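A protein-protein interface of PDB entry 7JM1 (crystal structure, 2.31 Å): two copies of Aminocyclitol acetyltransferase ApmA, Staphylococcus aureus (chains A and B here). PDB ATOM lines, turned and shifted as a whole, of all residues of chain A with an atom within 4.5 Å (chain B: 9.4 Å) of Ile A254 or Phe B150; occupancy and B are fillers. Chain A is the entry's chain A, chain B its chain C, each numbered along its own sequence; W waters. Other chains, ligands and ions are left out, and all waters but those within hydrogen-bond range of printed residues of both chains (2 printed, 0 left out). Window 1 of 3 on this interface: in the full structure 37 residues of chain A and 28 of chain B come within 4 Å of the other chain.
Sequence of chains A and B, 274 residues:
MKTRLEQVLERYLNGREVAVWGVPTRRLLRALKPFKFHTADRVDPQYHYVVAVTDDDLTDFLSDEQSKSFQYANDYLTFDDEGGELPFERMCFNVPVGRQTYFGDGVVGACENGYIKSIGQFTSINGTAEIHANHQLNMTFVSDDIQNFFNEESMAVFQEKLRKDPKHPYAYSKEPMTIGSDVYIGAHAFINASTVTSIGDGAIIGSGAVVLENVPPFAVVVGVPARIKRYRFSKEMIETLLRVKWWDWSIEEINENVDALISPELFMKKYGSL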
ATOM      1  N   PHE A 122       8.372   2.661 -10.855  1.00  0.00           N
ATOM      2  CA  PHE A 122       8.503   3.585  -9.727  1.00  0.00           C
ATOM      3  C   PHE A 122       7.446   3.324  -8.659  1.00  0.00           C
ATOM      4  O   PHE A 122       6.898   4.251  -8.059  1.00  0.00           O
ATOM      5  CB  PHE A 122       8.454   5.043 -10.197  1.00  0.00           C
ATOM      6  CG  PHE A 122       9.390   5.334 -11.336  1.00  0.00           C
ATOM      7  CD1 PHE A 122      10.752   5.454 -11.113  1.00  0.00           C
ATOM      8  CD2 PHE A 122       8.912   5.469 -12.630  1.00  0.00           C
ATOM      9  CE1 PHE A 122      11.623   5.703 -12.158  1.00  0.00           C
ATOM     10  CE2 PHE A 122       9.775   5.723 -13.680  1.00  0.00           C
ATOM     11  CZ  PHE A 122      11.135   5.838 -13.440  1.00  0.00           C
ATOM     12  N   TRP A 249       8.935   7.593 -19.168  1.00  0.00           N
ATOM     13  CA  TRP A 249       9.973   8.468 -19.700  1.00  0.00           C
ATOM     14  C   TRP A 249      11.354   7.836 -19.563  1.00  0.00           C
ATOM     15  O   TRP A 249      11.623   7.060 -18.642  1.00  0.00           O
ATOM     16  CB  TRP A 249       9.977   9.814 -18.971  1.00  0.00           C
ATOM     17  CG  TRP A 249       8.876  10.735 -19.377  1.00  0.00           C
ATOM     18  CD1 TRP A 249       8.048  10.592 -20.443  1.00  0.00           C
ATOM     19  CD2 TRP A 249       8.485  11.948 -18.722  1.00  0.00           C
ATOM     20  NE1 TRP A 249       7.155  11.637 -20.495  1.00  0.00           N
ATOM     21  CE2 TRP A 249       7.406  12.486 -19.448  1.00  0.00           C
ATOM     22  CE3 TRP A 249       8.945  12.632 -17.590  1.00  0.00           C
ATOM     23  CZ2 TRP A 249       6.779  13.675 -19.085  1.00  0.00           C
ATOM     24  CZ3 TRP A 249       8.314  13.810 -17.226  1.00  0.00           C
ATOM     25  CH2 TRP A 249       7.246  14.320 -17.977  1.00  0.00           C
ATOM     26  N   SER A 250      12.246   8.207 -20.479  1.00  0.00           N
ATOM     27  CA  SER A 250      13.641   7.828 -20.351  1.00  0.00           C
ATOM     28  C   SER A 250      14.285   8.588 -19.192  1.00  0.00           C
ATOM     29  O   SER A 250      13.715   9.527 -18.629  1.00  0.00           O
ATOM     30  CB  SER A 250      14.386   8.103 -21.654  1.00  0.00           C
ATOM     31  OG  SER A 250      14.599   9.495 -21.839  1.00  0.00           O
ATOM     32  N   ILE A 251      15.497   8.163 -18.831  1.00  0.00           N
ATOM     33  CA  ILE A 251      16.201   8.764 -17.700  1.00  0.00           C
ATOM     34  C   ILE A 251      16.475  10.242 -17.960  1.00  0.00           C
ATOM     35  O   ILE A 251      16.325  11.084 -17.064  1.00  0.00           O
ATOM     36  CB  ILE A 251      17.499   7.981 -17.411  1.00  0.00           C
ATOM     37  CG1 ILE A 251      17.183   6.652 -16.715  1.00  0.00           C
ATOM     38  CG2 ILE A 251      18.464   8.803 -16.571  1.00  0.00           C
ATOM     39  CD1 ILE A 251      18.346   5.671 -16.732  1.00  0.00           C
ATOM     40  N   GLU A 252      16.869  10.587 -19.186  1.00  0.00           N
ATOM     41  CA  GLU A 252      17.210  11.979 -19.465  1.00  0.00           C
ATOM     42  C   GLU A 252      15.984  12.886 -19.395  1.00  0.00           C
ATOM     43  O   GLU A 252      16.056  13.987 -18.833  1.00  0.00           O
ATOM     44  CB  GLU A 252      17.889  12.105 -20.828  1.00  0.00           C
ATOM     45  CG  GLU A 252      18.495  13.492 -21.076  1.00  0.00           C
ATOM     46  CD  GLU A 252      19.170  14.097 -19.835  1.00  0.00           C
ATOM     47  OE1 GLU A 252      19.985  13.406 -19.180  1.00  0.00           O
ATOM     48  OE2 GLU A 252      18.889  15.275 -19.520  1.00  0.00           O
ATOM     49  N   GLU A 253      14.850  12.452 -19.952  1.00  0.00           N
ATOM     50  CA  GLU A 253      13.684  13.329 -19.939  1.00  0.00           C
ATOM     51  C   GLU A 253      13.050  13.419 -18.556  1.00  0.00           C
ATOM     52  O   GLU A 253      12.334  14.385 -18.284  1.00  0.00           O
ATOM     53  CB  GLU A 253      12.649  12.884 -20.976  1.00  0.00           C
ATOM     54  CG  GLU A 253      12.318  11.418 -20.949  1.00  0.00           C
ATOM     55  CD  GLU A 253      11.680  10.947 -22.242  1.00  0.00           C
ATOM     56  OE1 GLU A 253      11.598  11.761 -23.179  1.00  0.00           O
ATOM     57  OE2 GLU A 253      11.264   9.773 -22.327  1.00  0.00           O
ATOM     58  N   ILE A 254      13.303  12.443 -17.679  1.00  0.00           N
ATOM     59  CA  ILE A 254      12.942  12.609 -16.275  1.00  0.00           C
ATOM     60  C   ILE A 254      13.748  13.747 -15.658  1.00  0.00           C
ATOM     61  O   ILE A 254      13.207  14.583 -14.923  1.00  0.00           O
ATOM     62  CB  ILE A 254      13.139  11.285 -15.510  1.00  0.00           C
ATOM     63  CG1 ILE A 254      11.994  10.314 -15.814  1.00  0.00           C
ATOM     64  CG2 ILE A 254      13.258  11.524 -13.990  1.00  0.00           C
ATOM     65  CD1 ILE A 254      12.270   8.881 -15.352  1.00  0.00           C
ATOM     66  N   ASN A 255      15.046  13.814 -15.967  1.00  0.00           N
ATOM     67  CA  ASN A 255      15.870  14.901 -15.450  1.00  0.00           C
ATOM     68  C   ASN A 255      15.498  16.235 -16.082  1.00  0.00           C
ATOM     69  O   ASN A 255      15.475  17.261 -15.394  1.00  0.00           O
ATOM     70  CB  ASN A 255      17.349  14.589 -15.667  1.00  0.00           C
ATOM     71  CG  ASN A 255      17.895  13.644 -14.616  1.00  0.00           C
ATOM     72  OD1 ASN A 255      18.289  14.070 -13.532  1.00  0.00           O
ATOM     73  ND2 ASN A 255      17.899  12.350 -14.922  1.00  0.00           N
ATOM     74  N   GLU A 256      15.197  16.240 -17.386  1.00  0.00           N
ATOM     75  CA  GLU A 256      14.771  17.470 -18.053  1.00  0.00           C
ATOM     76  C   GLU A 256      13.492  18.029 -17.445  1.00  0.00           C
ATOM     77  O   GLU A 256      13.300  19.250 -17.413  1.00  0.00           O
ATOM     78  CB  GLU A 256      14.543  17.222 -19.544  1.00  0.00           C
ATOM     79  CG  GLU A 256      15.781  16.971 -20.363  1.00  0.00           C
ATOM     80  CD  GLU A 256      15.561  17.296 -21.829  1.00  0.00           C
ATOM     81  OE1 GLU A 256      15.952  16.474 -22.689  1.00  0.00           O
ATOM     82  OE2 GLU A 256      14.993  18.374 -22.119  1.00  0.00           O
ATOM     83  N   ASN A 257      12.609  17.155 -16.961  1.00  0.00           N
ATOM     84  CA  ASN A 257      11.300  17.543 -16.447  1.00  0.00           C
ATOM     85  C   ASN A 257      11.233  17.517 -14.929  1.00  0.00           C
ATOM     86  O   ASN A 257      10.146  17.354 -14.366  1.00  0.00           O
ATOM     87  CB  ASN A 257      10.220  16.631 -17.027  1.00  0.00           C
ATOM     88  CG  ASN A 257       9.981  16.884 -18.502  1.00  0.00           C
ATOM     89  OD1 ASN A 257       9.102  17.663 -18.874  1.00  0.00           O
ATOM     90  ND2 ASN A 257      10.777  16.239 -19.350  1.00  0.00           N
ATOM     91  N   VAL A 258      12.373  17.676 -14.250  1.00  0.00           N
ATOM     92  CA  VAL A 258      12.374  17.523 -12.799  1.00  0.00           C
ATOM     93  C   VAL A 258      11.524  18.603 -12.141  1.00  0.00           C
ATOM     94  O   VAL A 258      10.905  18.363 -11.099  1.00  0.00           O
ATOM     95  CB  VAL A 258      13.819  17.513 -12.254  1.00  0.00           C
ATOM     96  CG1 VAL A 258      14.434  18.909 -12.287  1.00  0.00           C
ATOM     97  CG2 VAL A 258      13.841  16.956 -10.847  1.00  0.00           C
ATOM     98  N   LEU A 261       7.956  17.405 -12.562  1.00  0.00           N
ATOM     99  CA  LEU A 261       7.735  16.265 -11.681  1.00  0.00           C
ATOM    100  C   LEU A 261       7.660  16.698 -10.226  1.00  0.00           C
ATOM    101  O   LEU A 261       6.949  16.080  -9.426  1.00  0.00           O
ATOM    102  CB  LEU A 261       8.845  15.228 -11.868  1.00  0.00           C
ATOM    103  CG  LEU A 261       8.783  14.443 -13.177  1.00  0.00           C
ATOM    104  CD1 LEU A 261      10.053  13.645 -13.391  1.00  0.00           C
ATOM    105  CD2 LEU A 261       7.578  13.529 -13.163  1.00  0.00           C
ATOM    106  N   GLN B 136       7.229  12.068   0.070  1.00  0.00           N
ATOM    107  CA  GLN B 136       6.616  13.338  -0.305  1.00  0.00           C
ATOM    108  C   GLN B 136       5.215  13.097  -0.856  1.00  0.00           C
ATOM    109  O   GLN B 136       4.971  12.133  -1.585  1.00  0.00           O
ATOM    110  CB  GLN B 136       7.477  14.069  -1.340  1.00  0.00           C
ATOM    111  CG  GLN B 136       7.450  13.461  -2.732  1.00  0.00           C
ATOM    112  CD  GLN B 136       8.351  12.246  -2.847  1.00  0.00           C
ATOM    113  OE1 GLN B 136       9.178  11.986  -1.967  1.00  0.00           O
ATOM    114  NE2 GLN B 136       8.190  11.489  -3.928  1.00  0.00           N
ATOM    115  N   MET B 139       3.953  16.259  -4.563  1.00  0.00           N
ATOM    116  CA  MET B 139       4.718  16.297  -5.792  1.00  0.00           C
ATOM    117  C   MET B 139       3.931  15.518  -6.838  1.00  0.00           C
ATOM    118  O   MET B 139       2.925  14.884  -6.502  1.00  0.00           O
ATOM    119  CB  MET B 139       6.098  15.698  -5.543  1.00  0.00           C
ATOM    120  CG  MET B 139       6.995  16.608  -4.718  1.00  0.00           C
ATOM    121  SD  MET B 139       8.881  16.271  -5.043  1.00  0.00           S
ATOM    122  CE  MET B 139       9.582  16.136  -3.308  1.00  0.00           C
ATOM    123  N   PHE B 141       4.951  12.886  -8.332  1.00  0.00           N
ATOM    124  CA  PHE B 141       5.243  11.488  -8.061  1.00  0.00           C
ATOM    125  C   PHE B 141       5.292  11.249  -6.559  1.00  0.00           C
ATOM    126  O   PHE B 141       5.531  12.168  -5.767  1.00  0.00           O
ATOM    127  CB  PHE B 141       6.574  11.072  -8.703  1.00  0.00           C
ATOM    128  CG  PHE B 141       7.764  11.848  -8.201  1.00  0.00           C
ATOM    129  CD1 PHE B 141       8.073  13.095  -8.725  1.00  0.00           C
ATOM    130  CD2 PHE B 141       8.584  11.320  -7.209  1.00  0.00           C
ATOM    131  CE1 PHE B 141       9.179  13.808  -8.265  1.00  0.00           C
ATOM    132  CE2 PHE B 141       9.690  12.026  -6.746  1.00  0.00           C
ATOM    133  CZ  PHE B 141       9.990  13.265  -7.270  1.00  0.00           C
ATOM    134  N   SER B 143       6.957   8.130  -5.640  1.00  0.00           N
ATOM    135  CA  SER B 143       8.117   7.254  -5.561  1.00  0.00           C
ATOM    136  C   SER B 143       9.286   7.919  -4.843  1.00  0.00           C
ATOM    137  O   SER B 143       9.508   9.130  -4.941  1.00  0.00           O
ATOM    138  CB  SER B 143       8.556   6.855  -6.974  1.00  0.00           C
ATOM    139  OG  SER B 143       9.799   6.182  -6.946  1.00  0.00           O
ATOM    140  N   ASP B 144      10.057   7.106  -4.129  1.00  0.00           N
ATOM    141  CA  ASP B 144      11.357   7.546  -3.642  1.00  0.00           C
ATOM    142  C   ASP B 144      12.507   7.064  -4.517  1.00  0.00           C
ATOM    143  O   ASP B 144      13.455   7.817  -4.745  1.00  0.00           O
ATOM    144  CB  ASP B 144      11.578   7.089  -2.195  1.00  0.00           C
ATOM    145  CG  ASP B 144      11.503   5.580  -2.033  1.00  0.00           C
ATOM    146  OD1 ASP B 144      10.936   4.899  -2.915  1.00  0.00           O
ATOM    147  OD2 ASP B 144      11.993   5.077  -1.001  1.00  0.00           O
ATOM    148  N   ASP B 145      12.436   5.842  -5.050  1.00  0.00           N
ATOM    149  CA  ASP B 145      13.565   5.290  -5.797  1.00  0.00           C
ATOM    150  C   ASP B 145      13.766   5.937  -7.158  1.00  0.00           C
ATOM    151  O   ASP B 145      14.809   5.703  -7.780  1.00  0.00           O
ATOM    152  CB  ASP B 145      13.396   3.784  -5.969  1.00  0.00           C
ATOM    153  CG  ASP B 145      13.888   3.014  -4.767  1.00  0.00           C
ATOM    154  OD1 ASP B 145      14.110   3.651  -3.713  1.00  0.00           O
ATOM    155  OD2 ASP B 145      14.055   1.782  -4.872  1.00  0.00           O
ATOM    156  N   ILE B 146      12.805   6.733  -7.639  1.00  0.00           N
ATOM    157  CA  ILE B 146      13.021   7.518  -8.852  1.00  0.00           C
ATOM    158  C   ILE B 146      14.248   8.408  -8.706  1.00  0.00           C
ATOM    159  O   ILE B 146      14.915   8.731  -9.696  1.00  0.00           O
ATOM    160  CB  ILE B 146      11.759   8.343  -9.178  1.00  0.00           C
ATOM    161  CG1 ILE B 146      11.893   9.064 -10.519  1.00  0.00           C
ATOM    162  CG2 ILE B 146      11.479   9.352  -8.077  1.00  0.00           C
ATOM    163  CD1 ILE B 146      10.715   9.983 -10.808  1.00  0.00           C
ATOM    164  N   GLN B 147      14.587   8.794  -7.474  1.00  0.00           N
ATOM    165  CA  GLN B 147      15.742   9.652  -7.246  1.00  0.00           C
ATOM    166  C   GLN B 147      17.059   8.974  -7.594  1.00  0.00           C
ATOM    167  O   GLN B 147      18.076   9.667  -7.697  1.00  0.00           O
ATOM    168  CB  GLN B 147      15.774  10.122  -5.794  1.00  0.00           C
ATOM    169  CG  GLN B 147      16.271   9.084  -4.816  1.00  0.00           C
ATOM    170  CD  GLN B 147      16.083   9.524  -3.389  1.00  0.00           C
ATOM    171  OE1 GLN B 147      16.659  10.520  -2.960  1.00  0.00           O
ATOM    172  NE2 GLN B 147      15.264   8.791  -2.643  1.00  0.00           N
ATOM    173  N   ASN B 148      17.065   7.649  -7.769  1.00  0.00           N
ATOM    174  CA  ASN B 148      18.232   6.961  -8.306  1.00  0.00           C
ATOM    175  C   ASN B 148      18.492   7.311  -9.767  1.00  0.00           C
ATOM    176  O   ASN B 148      19.585   7.025 -10.269  1.00  0.00           O
ATOM    177  CB  ASN B 148      18.067   5.445  -8.157  1.00  0.00           C
ATOM    178  CG  ASN B 148      17.970   5.005  -6.707  1.00  0.00           C
ATOM    179  OD1 ASN B 148      18.580   5.604  -5.822  1.00  0.00           O
ATOM    180  ND2 ASN B 148      17.196   3.954  -6.455  1.00  0.00           N
ATOM    181  N   PHE B 149      17.527   7.922 -10.458  1.00  0.00           N
ATOM    182  CA  PHE B 149      17.729   8.411 -11.816  1.00  0.00           C
ATOM    183  C   PHE B 149      18.075   9.895 -11.878  1.00  0.00           C
ATOM    184  O   PHE B 149      18.454  10.378 -12.949  1.00  0.00           O
ATOM    185  CB  PHE B 149      16.476   8.148 -12.670  1.00  0.00           C
ATOM    186  CG  PHE B 149      16.305   6.706 -13.060  1.00  0.00           C
ATOM    187  CD1 PHE B 149      17.366   5.814 -12.951  1.00  0.00           C
ATOM    188  CD2 PHE B 149      15.088   6.239 -13.533  1.00  0.00           C
ATOM    189  CE1 PHE B 149      17.219   4.482 -13.310  1.00  0.00           C
ATOM    190  CE2 PHE B 149      14.929   4.903 -13.898  1.00  0.00           C
ATOM    191  CZ  PHE B 149      15.996   4.026 -13.784  1.00  0.00           C
ATOM    192  N   PHE B 150      17.960  10.628 -10.771  1.00  0.00           N
ATOM    193  CA  PHE B 150      18.269  12.055 -10.790  1.00  0.00           C
ATOM    194  C   PHE B 150      19.774  12.279 -10.847  1.00  0.00           C
ATOM    195  O   PHE B 150      20.524  11.723 -10.037  1.00  0.00           O
ATOM    196  CB  PHE B 150      17.705  12.744  -9.547  1.00  0.00           C
ATOM    197  CG  PHE B 150      16.212  12.831  -9.521  1.00  0.00           C
ATOM    198  CD1 PHE B 150      15.473  12.681 -10.685  1.00  0.00           C
ATOM    199  CD2 PHE B 150      15.545  13.073  -8.334  1.00  0.00           C
ATOM    200  CE1 PHE B 150      14.099  12.759 -10.663  1.00  0.00           C
ATOM    201  CE2 PHE B 150      14.163  13.154  -8.304  1.00  0.00           C
ATOM    202  CZ  PHE B 150      13.439  12.995  -9.471  1.00  0.00           C
ATOM    203  N   ASN B 151      20.225  13.114 -11.782  1.00  0.00           N
ATOM    204  CA  ASN B 151      21.613  13.538 -11.706  1.00  0.00           C
ATOM    205  C   ASN B 151      21.792  14.524 -10.548  1.00  0.00           C
ATOM    206  O   ASN B 151      20.874  14.800  -9.768  1.00  0.00           O
ATOM    207  CB  ASN B 151      22.090  14.129 -13.034  1.00  0.00           C
ATOM    208  CG  ASN B 151      21.239  15.284 -13.516  1.00  0.00           C
ATOM    209  OD1 ASN B 151      20.857  16.165 -12.744  1.00  0.00           O
ATOM    210  ND2 ASN B 151      20.951  15.295 -14.813  1.00  0.00           N
ATOM    211  N   GLU B 152      23.004  15.058 -10.437  1.00  0.00           N
ATOM    212  CA  GLU B 152      23.353  15.877  -9.283  1.00  0.00           C
ATOM    213  C   GLU B 152      22.488  17.127  -9.212  1.00  0.00           C
ATOM    214  O   GLU B 152      22.035  17.520  -8.131  1.00  0.00           O
ATOM    215  CB  GLU B 152      24.838  16.245  -9.335  1.00  0.00           C
ATOM    216  CG  GLU B 152      25.787  15.039  -9.347  1.00  0.00           C
ATOM    217  CD  GLU B 152      25.685  14.188 -10.614  1.00  0.00           C
ATOM    218  OE1 GLU B 152      26.092  13.008 -10.571  1.00  0.00           O
ATOM    219  OE2 GLU B 152      25.186  14.696 -11.644  1.00  0.00           O
ATOM    220  N   GLU B 153      22.220  17.753 -10.357  1.00  0.00           N
ATOM    221  CA  GLU B 153      21.414  18.964 -10.329  1.00  0.00           C
ATOM    222  C   GLU B 153      19.956  18.658  -9.995  1.00  0.00           C
ATOM    223  O   GLU B 153      19.358  19.345  -9.161  1.00  0.00           O
ATOM    224  CB  GLU B 153      21.531  19.719 -11.651  1.00  0.00           C
ATOM    225  CG  GLU B 153      21.196  21.195 -11.512  1.00  0.00           C
ATOM    226  CD  GLU B 153      21.834  21.829 -10.279  1.00  0.00           C
ATOM    227  OE1 GLU B 153      21.093  22.172  -9.329  1.00  0.00           O
ATOM    228  OE2 GLU B 153      23.076  21.986 -10.259  1.00  0.00           O
ATOM    229  N   SER B 154      19.370  17.623 -10.610  1.00  0.00           N
ATOM    230  CA  SER B 154      17.992  17.274 -10.265  1.00  0.00           C
ATOM    231  C   SER B 154      17.873  16.870  -8.802  1.00  0.00           C
ATOM    232  O   SER B 154      16.904  17.236  -8.126  1.00  0.00           O
ATOM    233  CB  SER B 154      17.445  16.162 -11.169  1.00  0.00           C
ATOM    234  OG  SER B 154      17.780  16.341 -12.534  1.00  0.00           O
ATOM    235  N   MET B 155      18.850  16.124  -8.295  1.00  0.00           N
ATOM    236  CA  MET B 155      18.847  15.699  -6.900  1.00  0.00           C
ATOM    237  C   MET B 155      18.865  16.917  -5.980  1.00  0.00           C
ATOM    238  O   MET B 155      18.138  16.962  -4.988  1.00  0.00           O
ATOM    239  CB  MET B 155      20.051  14.800  -6.598  1.00  0.00           C
ATOM    240  CG  MET B 155      20.096  14.306  -5.166  1.00  0.00           C
ATOM    241  SD  MET B 155      18.440  13.381  -4.672  1.00  0.00           S
ATOM    242  CE  MET B 155      18.906  11.606  -5.188  1.00  0.00           C
ATOM    243  N   ALA B 156      19.702  17.900  -6.325  1.00  0.00           N
ATOM    244  CA  ALA B 156      19.766  19.136  -5.553  1.00  0.00           C
ATOM    245  C   ALA B 156      18.401  19.816  -5.495  1.00  0.00           C
ATOM    246  O   ALA B 156      17.899  20.119  -4.409  1.00  0.00           O
ATOM    247  CB  ALA B 156      20.815  20.080  -6.150  1.00  0.00           C
ATOM    248  N   VAL B 157      17.794  20.055  -6.665  1.00  0.00           N
ATOM    249  CA  VAL B 157      16.428  20.584  -6.722  1.00  0.00           C
ATOM    250  C   VAL B 157      15.501  19.768  -5.840  1.00  0.00           C
ATOM    251  O   VAL B 157      14.722  20.312  -5.040  1.00  0.00           O
ATOM    252  CB  VAL B 157      15.936  20.600  -8.184  1.00  0.00           C
ATOM    253  CG1 VAL B 157      14.660  21.397  -8.309  1.00  0.00           C
ATOM    254  CG2 VAL B 157      16.988  21.173  -9.099  1.00  0.00           C
ATOM    255  N   PHE B 158      15.566  18.443  -5.953  1.00  0.00           N
ATOM    256  CA  PHE B 158      14.678  17.558  -5.219  1.00  0.00           C
ATOM    257  C   PHE B 158      14.893  17.683  -3.711  1.00  0.00           C
ATOM    258  O   PHE B 158      13.935  17.780  -2.939  1.00  0.00           O
ATOM    259  CB  PHE B 158      14.918  16.128  -5.698  1.00  0.00           C
ATOM    260  CG  PHE B 158      14.138  15.081  -4.973  1.00  0.00           C
ATOM    261  CD1 PHE B 158      12.748  15.057  -5.016  1.00  0.00           C
ATOM    262  CD2 PHE B 158      14.800  14.077  -4.291  1.00  0.00           C
ATOM    263  CE1 PHE B 158      12.037  14.052  -4.364  1.00  0.00           C
ATOM    264  CE2 PHE B 158      14.098  13.072  -3.638  1.00  0.00           C
ATOM    265  CZ  PHE B 158      12.717  13.058  -3.675  1.00  0.00           C
ATOM    266  N   GLN B 159      16.158  17.703  -3.284  1.00  0.00           N
ATOM    267  CA  GLN B 159      16.449  17.785  -1.856  1.00  0.00           C
ATOM    268  C   GLN B 159      16.039  19.136  -1.286  1.00  0.00           C
ATOM    269  O   GLN B 159      15.559  19.210  -0.149  1.00  0.00           O
ATOM    270  CB  GLN B 159      17.934  17.525  -1.609  1.00  0.00           C
ATOM    271  CG  GLN B 159      18.376  16.105  -1.918  1.00  0.00           C
ATOM    272  CD  GLN B 159      17.807  15.098  -0.947  1.00  0.00           C
ATOM    273  OE1 GLN B 159      17.394  14.005  -1.338  1.00  0.00           O
ATOM    274  NE2 GLN B 159      17.782  15.460   0.330  1.00  0.00           N
ATOM    275  N   LEU B 162      12.295  18.971  -0.617  1.00  0.00           N
ATOM    276  CA  LEU B 162      11.970  18.097   0.507  1.00  0.00           C
ATOM    277  C   LEU B 162      12.209  18.805   1.839  1.00  0.00           C
ATOM    278  O   LEU B 162      11.450  18.618   2.797  1.00  0.00           O
ATOM    279  CB  LEU B 162      12.789  16.812   0.435  1.00  0.00           C
ATOM    280  CG  LEU B 162      12.391  15.804  -0.641  1.00  0.00           C
ATOM    281  CD1 LEU B 162      13.320  14.608  -0.585  1.00  0.00           C
ATOM    282  CD2 LEU B 162      10.961  15.367  -0.437  1.00  0.00           C
ATOM    283  N   TYR B 170      10.242  11.894   4.777  1.00  0.00           N
ATOM    284  CA  TYR B 170      11.484  11.260   5.206  1.00  0.00           C
ATOM    285  C   TYR B 170      12.018  11.863   6.502  1.00  0.00           C
ATOM    286  O   TYR B 170      13.221  11.794   6.769  1.00  0.00           O
ATOM    287  CB  TYR B 170      12.546  11.324   4.096  1.00  0.00           C
ATOM    288  CG  TYR B 170      11.987  10.920   2.750  1.00  0.00           C
ATOM    289  CD1 TYR B 170      11.776   9.579   2.440  1.00  0.00           C
ATOM    290  CD2 TYR B 170      11.633  11.877   1.805  1.00  0.00           C
ATOM    291  CE1 TYR B 170      11.244   9.199   1.219  1.00  0.00           C
ATOM    292  CE2 TYR B 170      11.097  11.509   0.579  1.00  0.00           C
ATOM    293  CZ  TYR B 170      10.906  10.170   0.292  1.00  0.00           C
ATOM    294  OH  TYR B 170      10.377   9.795  -0.924  1.00  0.00           O
HETATM  295  O   HOH W   1       6.115   4.813  -5.497  1.00  0.00           O
HETATM  296  O   HOH W   2      21.092  13.892 -16.779  1.00  0.00           O
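The backbone carbonyl oxygen (O) of Phe B141 sits close to the side-chain amide nitrogen (NE2) of Gln B136, at 3.3 Å. The side-chain amide nitrogen (NE2) of Gln B136 sits at hydrogen-bond distance from the backbone carbonyl oxygen (O) of Ser B143, 2.9 Å away. N of Asp B145 sits at hydrogen-bond distance from OG of Ser B143 (3.3 Å). OG of Ser B143 lies within hydrogen-bond range of N of Ile B146 (3.1 Å). The side-chain amide oxygen (OD1) of Asn B151 lies within hydrogen-bond range of the backbone NH (N) of Glu B153 (3.2 Å). The backbone NH (N) of Ser B154 is in hydrogen-bond range of the side-chain amide oxygen (OD1) of Asn B151 (3.0 Å).
Ile A254 touches one residue of chain B. Of chain B, only Phe B149 (2.8 Å), Phe B150 (3.4 Å), Asn B151 (2.8 Å) and Ser B154 (2.5 Å) come within 4 Å of Asn A255. Glu A256 touches none of the printed residues of chain B. Printed residues of chain B within 4 Å of Leu A261: Met B139 and Phe B141. Phe B150 touches just these residues of chain A: Ile A254 (3.6 Å) and Asn A255 (3.4 Å). Of the printed residues of chain A, Ser B154 touches Asn A255 (2.5 Å) and Val A258 (3.7 Å). The nearest residue of chain A that does not touch Phe B150 is Val A258 (4.2 Å).
No position is printed for both chains.
The side-chain amide nitrogen (ND2) of Asn A255 lies within hydrogen-bond range of the backbone carbonyl oxygen (O) of Phe B149 (2.8 Å). The backbone NH (N) of Asn B151 lies within hydrogen-bond range of the side-chain amide oxygen (OD1) of Asn A255 (2.8 Å). OG of Ser B154 sits at hydrogen-bond distance from OD1 of Asn A255 (2.5 Å).
Among the printed residues, merely in contact across the chains: Leu A261 with Phe B141, Phe A122 with Ser B143, Asn A255 with Phe B150, Phe A122 with Ile B146, Ile A254 with Phe B150, Val A258 with Ser B154, Ile A251 with Phe B149, Phe A122 with Phe B149 and Leu A261 with Met B139.
Water W2 lies within hydrogen-bond range of the side-chain amide nitrogen (ND2) of Asn B151 (2.4 Å) and the side-chain carboxylate (OE1) of Glu A252 (2.7 Å). Water W1 lies within hydrogen-bond range of O of Phe A122 (2.7 Å) and N of Ser B143 (3.4 Å).
Printed residues of chain A that touch a printed residue of chain B: Phe A122, Ile A251, Ile A254, Asn A255, Val A258 and Leu A261. Hydrophobic or aromatic side chains of chain B within 4 Å of the printed part of chain A: Met B139, Phe B141, Ile B146, Phe B149 and Phe B150.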
